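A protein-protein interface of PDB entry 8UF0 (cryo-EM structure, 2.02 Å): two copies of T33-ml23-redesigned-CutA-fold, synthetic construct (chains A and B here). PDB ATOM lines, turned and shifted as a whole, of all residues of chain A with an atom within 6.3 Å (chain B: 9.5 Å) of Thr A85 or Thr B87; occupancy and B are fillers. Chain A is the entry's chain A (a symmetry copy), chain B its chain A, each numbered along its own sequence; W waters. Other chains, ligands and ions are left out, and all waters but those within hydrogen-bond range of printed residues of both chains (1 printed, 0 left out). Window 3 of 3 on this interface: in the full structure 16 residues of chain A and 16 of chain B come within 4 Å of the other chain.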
ATOM      1  N   ALA A   2      24.063  14.665  20.738  1.00  0.00           N
ATOM      2  CA  ALA A   2      23.598  15.694  19.820  1.00  0.00           C
ATOM      3  C   ALA A   2      23.981  17.101  20.293  1.00  0.00           C
ATOM      4  O   ALA A   2      24.042  17.362  21.487  1.00  0.00           O
ATOM      5  CB  ALA A   2      22.099  15.583  19.639  1.00  0.00           C
ATOM      6  N   ILE A   3      24.223  17.996  19.340  1.00  0.00           N
ATOM      7  CA  ILE A   3      24.647  19.368  19.603  1.00  0.00           C
ATOM      8  C   ILE A   3      23.674  20.327  18.920  1.00  0.00           C
ATOM      9  O   ILE A   3      23.377  20.168  17.734  1.00  0.00           O
ATOM     10  CB  ILE A   3      26.086  19.608  19.111  1.00  0.00           C
ATOM     11  CG1 ILE A   3      27.062  18.658  19.803  1.00  0.00           C
ATOM     12  CG2 ILE A   3      26.511  21.042  19.330  1.00  0.00           C
ATOM     13  CD1 ILE A   3      28.346  18.493  19.060  1.00  0.00           C
ATOM     14  N   GLU A  60      19.977  12.217  22.091  1.00  0.00           N
ATOM     15  CA  GLU A  60      19.269  12.200  20.813  1.00  0.00           C
ATOM     16  C   GLU A  60      17.752  12.150  20.990  1.00  0.00           C
ATOM     17  O   GLU A  60      17.013  12.787  20.236  1.00  0.00           O
ATOM     18  CB  GLU A  60      19.750  11.016  19.981  1.00  0.00           C
ATOM     19  CG  GLU A  60      19.046  10.872  18.663  1.00  0.00           C
ATOM     20  CD  GLU A  60      19.335  12.020  17.733  1.00  0.00           C
ATOM     21  OE1 GLU A  60      20.512  12.207  17.361  1.00  0.00           O
ATOM     22  OE2 GLU A  60      18.384  12.745  17.372  1.00  0.00           O
ATOM     23  N   ILE A  82      20.128  25.005  14.693  1.00  0.00           N
ATOM     24  CA  ILE A  82      20.805  24.002  13.877  1.00  0.00           C
ATOM     25  C   ILE A  82      21.240  22.827  14.751  1.00  0.00           C
ATOM     26  O   ILE A  82      21.692  23.022  15.881  1.00  0.00           O
ATOM     27  CB  ILE A  82      22.003  24.642  13.140  1.00  0.00           C
ATOM     28  CG1 ILE A  82      21.508  25.427  11.933  1.00  0.00           C
ATOM     29  CG2 ILE A  82      23.014  23.622  12.704  1.00  0.00           C
ATOM     30  CD1 ILE A  82      22.246  26.695  11.710  1.00  0.00           C
ATOM     31  N   VAL A  83      21.104  21.606  14.226  1.00  0.00           N
ATOM     32  CA  VAL A  83      21.395  20.373  14.955  1.00  0.00           C
ATOM     33  C   VAL A  83      22.496  19.594  14.233  1.00  0.00           C
ATOM     34  O   VAL A  83      22.418  19.388  13.021  1.00  0.00           O
ATOM     35  CB  VAL A  83      20.133  19.498  15.112  1.00  0.00           C
ATOM     36  CG1 VAL A  83      20.438  18.244  15.905  1.00  0.00           C
ATOM     37  CG2 VAL A  83      19.001  20.274  15.763  1.00  0.00           C
ATOM     38  N   ILE A  84      23.500  19.137  14.986  1.00  0.00           N
ATOM     39  CA  ILE A  84      24.630  18.369  14.459  1.00  0.00           C
ATOM     40  C   ILE A  84      24.754  17.054  15.226  1.00  0.00           C
ATOM     41  O   ILE A  84      24.683  17.043  16.459  1.00  0.00           O
ATOM     42  CB  ILE A  84      25.945  19.170  14.549  1.00  0.00           C
ATOM     43  CG1 ILE A  84      25.952  20.306  13.535  1.00  0.00           C
ATOM     44  CG2 ILE A  84      27.157  18.281  14.335  1.00  0.00           C
ATOM     45  CD1 ILE A  84      26.913  21.388  13.869  1.00  0.00           C
ATOM     46  N   THR A  85      24.953  15.953  14.503  1.00  0.00           N
ATOM     47  CA  THR A  85      25.073  14.615  15.089  1.00  0.00           C
ATOM     48  C   THR A  85      26.513  14.106  15.048  1.00  0.00           C
ATOM     49  O   THR A  85      27.025  13.808  13.962  1.00  0.00           O
ATOM     50  CB  THR A  85      24.152  13.634  14.359  1.00  0.00           C
ATOM     51  OG1 THR A  85      22.794  14.065  14.478  1.00  0.00           O
ATOM     52  CG2 THR A  85      24.283  12.236  14.943  1.00  0.00           C
ATOM     53  N   PRO A  86      27.190  13.962  16.185  1.00  0.00           N
ATOM     54  CA  PRO A  86      28.572  13.463  16.175  1.00  0.00           C
ATOM     55  C   PRO A  86      28.666  11.989  15.808  1.00  0.00           C
ATOM     56  O   PRO A  86      27.754  11.202  16.060  1.00  0.00           O
ATOM     57  CB  PRO A  86      29.044  13.694  17.615  1.00  0.00           C
ATOM     58  CG  PRO A  86      28.002  14.551  18.248  1.00  0.00           C
ATOM     59  CD  PRO A  86      26.735  14.285  17.543  1.00  0.00           C
ATOM     60  N   THR A  87      29.803  11.616  15.215  1.00  0.00           N
ATOM     61  CA  THR A  87      30.042  10.240  14.786  1.00  0.00           C
ATOM     62  C   THR A  87      30.631   9.346  15.874  1.00  0.00           C
ATOM     63  O   THR A  87      30.619   8.126  15.708  1.00  0.00           O
ATOM     64  CB  THR A  87      30.975  10.190  13.557  1.00  0.00           C
ATOM     65  OG1 THR A  87      31.978  11.205  13.647  1.00  0.00           O
ATOM     66  CG2 THR A  87      30.192  10.379  12.274  1.00  0.00           C
ATOM     67  N   ALA B   2      23.892  24.045   4.927  1.00  0.00           N
ATOM     68  CA  ALA B   2      25.309  23.711   4.905  1.00  0.00           C
ATOM     69  C   ALA B   2      26.165  24.799   5.561  1.00  0.00           C
ATOM     70  O   ALA B   2      25.837  25.977   5.492  1.00  0.00           O
ATOM     71  CB  ALA B   2      25.758  23.467   3.479  1.00  0.00           C
ATOM     72  N   ILE B   3      27.267  24.387   6.182  1.00  0.00           N
ATOM     73  CA  ILE B   3      28.174  25.275   6.901  1.00  0.00           C
ATOM     74  C   ILE B   3      29.584  25.105   6.339  1.00  0.00           C
ATOM     75  O   ILE B   3      30.067  23.978   6.209  1.00  0.00           O
ATOM     76  CB  ILE B   3      28.151  24.985   8.414  1.00  0.00           C
ATOM     77  CG1 ILE B   3      26.744  25.169   8.979  1.00  0.00           C
ATOM     78  CG2 ILE B   3      29.129  25.865   9.158  1.00  0.00           C
ATOM     79  CD1 ILE B   3      26.538  24.463  10.278  1.00  0.00           C
ATOM     80  N   ILE B  84      30.379  21.072   6.504  1.00  0.00           N
ATOM     81  CA  ILE B  84      29.618  20.270   7.465  1.00  0.00           C
ATOM     82  C   ILE B  84      28.133  20.328   7.112  1.00  0.00           C
ATOM     83  O   ILE B  84      27.600  21.408   6.840  1.00  0.00           O
ATOM     84  CB  ILE B  84      29.846  20.755   8.911  1.00  0.00           C
ATOM     85  CG1 ILE B  84      31.250  20.398   9.381  1.00  0.00           C
ATOM     86  CG2 ILE B  84      28.820  20.172   9.865  1.00  0.00           C
ATOM     87  CD1 ILE B  84      31.717  21.223  10.524  1.00  0.00           C
ATOM     88  N   THR B  85      27.465  19.175   7.131  1.00  0.00           N
ATOM     89  CA  THR B  85      26.042  19.063   6.798  1.00  0.00           C
ATOM     90  C   THR B  85      25.188  18.818   8.040  1.00  0.00           C
ATOM     91  O   THR B  85      25.261  17.730   8.627  1.00  0.00           O
ATOM     92  CB  THR B  85      25.824  17.937   5.784  1.00  0.00           C
ATOM     93  OG1 THR B  85      26.553  18.216   4.586  1.00  0.00           O
ATOM     94  CG2 THR B  85      24.348  17.794   5.446  1.00  0.00           C
ATOM     95  N   PRO B  86      24.354  19.767   8.460  1.00  0.00           N
ATOM     96  CA  PRO B  86      23.512  19.551   9.646  1.00  0.00           C
ATOM     97  C   PRO B  86      22.405  18.535   9.409  1.00  0.00           C
ATOM     98  O   PRO B  86      21.913  18.366   8.294  1.00  0.00           O
ATOM     99  CB  PRO B  86      22.923  20.940   9.920  1.00  0.00           C
ATOM    100  CG  PRO B  86      23.686  21.881   9.050  1.00  0.00           C
ATOM    101  CD  PRO B  86      24.164  21.106   7.890  1.00  0.00           C
ATOM    102  N   THR B  87      22.003  17.860  10.489  1.00  0.00           N
ATOM    103  CA  THR B  87      20.961  16.838  10.427  1.00  0.00           C
ATOM    104  C   THR B  87      19.545  17.388  10.574  1.00  0.00           C
ATOM    105  O   THR B  87      18.595  16.666  10.269  1.00  0.00           O
ATOM    106  CB  THR B  87      21.177  15.751  11.500  1.00  0.00           C
ATOM    107  OG1 THR B  87      21.681  16.331  12.707  1.00  0.00           O
ATOM    108  CG2 THR B  87      22.146  14.693  11.016  1.00  0.00           C
ATOM    109  N   ASP B  88      19.377  18.633  11.009  1.00  0.00           N
ATOM    110  CA  ASP B  88      18.054  19.207  11.228  1.00  0.00           C
ATOM    111  C   ASP B  88      18.196  20.712  11.416  1.00  0.00           C
ATOM    112  O   ASP B  88      19.275  21.205  11.751  1.00  0.00           O
ATOM    113  CB  ASP B  88      17.370  18.571  12.443  1.00  0.00           C
ATOM    114  CG  ASP B  88      15.867  18.576  12.334  1.00  0.00           C
ATOM    115  OD1 ASP B  88      15.344  18.354  11.223  1.00  0.00           O
ATOM    116  OD2 ASP B  88      15.200  18.804  13.362  1.00  0.00           O
ATOM    117  N   ALA B  89      17.091  21.432  11.207  1.00  0.00           N
ATOM    118  CA  ALA B  89      17.052  22.890  11.310  1.00  0.00           C
ATOM    119  C   ALA B  89      15.604  23.363  11.377  1.00  0.00           C
ATOM    120  O   ALA B  89      14.694  22.683  10.899  1.00  0.00           O
ATOM    121  CB  ALA B  89      17.776  23.550  10.133  1.00  0.00           C
ATOM    122  N   ASN B  90      15.406  24.542  11.965  1.00  0.00           N
ATOM    123  CA  ASN B  90      14.102  25.203  12.019  1.00  0.00           C
ATOM    124  C   ASN B  90      13.609  25.489  10.602  1.00  0.00           C
ATOM    125  O   ASN B  90      14.293  26.192   9.851  1.00  0.00           O
ATOM    126  CB  ASN B  90      14.220  26.501  12.829  1.00  0.00           C
ATOM    127  CG  ASN B  90      12.926  27.316  12.872  1.00  0.00           C
ATOM    128  OD1 ASN B  90      11.841  26.816  12.604  1.00  0.00           O
ATOM    129  ND2 ASN B  90      13.050  28.582  13.224  1.00  0.00           N
ATOM    130  N   LYS B  94      15.184  27.954   7.193  1.00  0.00           N
ATOM    131  CA  LYS B  94      15.528  27.502   5.847  1.00  0.00           C
ATOM    132  C   LYS B  94      14.794  28.306   4.784  1.00  0.00           C
ATOM    133  O   LYS B  94      15.344  28.576   3.714  1.00  0.00           O
ATOM    134  CB  LYS B  94      15.235  26.014   5.683  1.00  0.00           C
ATOM    135  CG  LYS B  94      16.303  25.136   6.263  1.00  0.00           C
ATOM    136  CD  LYS B  94      15.740  23.891   6.881  1.00  0.00           C
ATOM    137  CE  LYS B  94      15.504  22.838   5.834  1.00  0.00           C
ATOM    138  NZ  LYS B  94      16.728  22.611   5.026  1.00  0.00           N
HETATM  139  O   HOH W   1      25.268  16.469  11.379  1.00  0.00           O
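Of the 9 printed residues of chain A, 4 touch a printed residue of chain B. Printed residues of chain A that touch a printed residue of chain B: Ile A82, Val A83, Ile A84 and Thr A85. Hydrophobic or aromatic side chains of chain A that line the printed part of chain B: Ile A82 and Val A83. Among the printed residues, no Asp or Glu carboxylate lies within 4 Å of a Lys or Arg side-chain nitrogen of the other chain.
Among the printed residues, pairs that only touch across the chains: Val A83 with Pro B86 (3.5 Å), Ile A82 with Asp B88 (3.8 Å), Ile A82 with Pro B86 (3.9 Å) and Ile A84 with Thr B87 (3.99 Å).
The backbone NH of Ile A84 is in hydrogen-bond range of the backbone carbonyl oxygen of Ile A3 (2.9 Å).
The side-chain hydroxyl (OG1) of Thr B87 lies within hydrogen-bond range of the side-chain hydroxyl (OG1) of Thr A85. The backbone NH (N) of Val A83 is in hydrogen-bond range of the backbone carbonyl oxygen (O) of Asp B88, at 3.1 Å. The backbone NH of Thr B87 is in hydrogen-bond range of the backbone carbonyl oxygen of Val A83.
Of the printed residues of chain B, Ile A84 touches Thr B87. Thr A85 touches just one residue of chain B: Thr B87 (3.1 Å). No residue of chain B comes within 4 Å of Pro A86. Printed residues of chain A within 4 Å of Pro B86: Ile A82 (3.9 Å) and Val A83 (3.5 Å). Of the printed residues of chain A, Thr B87 touches Val A83 (3.0 Å), Ile A84 (3.99 Å) and Thr A85 (3.1 Å). Of the printed residues of chain A, Asp B88 touches Ile A82 (3.8 Å) and Val A83 (3.1 Å). Ala B89 touches none of the printed residues of chain A. Lys B94 touches none of the printed residues of chain A. The nearest printed residue of chain A that does not touch Thr B87 is Ile A82 (6.3 Å).
Ile A84 touches Thr B87, but with the chains exchanged Thr A87 does not touch Ile B84 (10.1 Å). Thr A85 touches Thr B87, but with the chains exchanged Thr A87 does not touch Thr B85 (9.6 Å). Of the 7 pairs that touch across the chains among the printed residues, none has its exchanged pair printed and touching as well.
Water W1 bridges O of Thr B85 and N of Thr A85.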
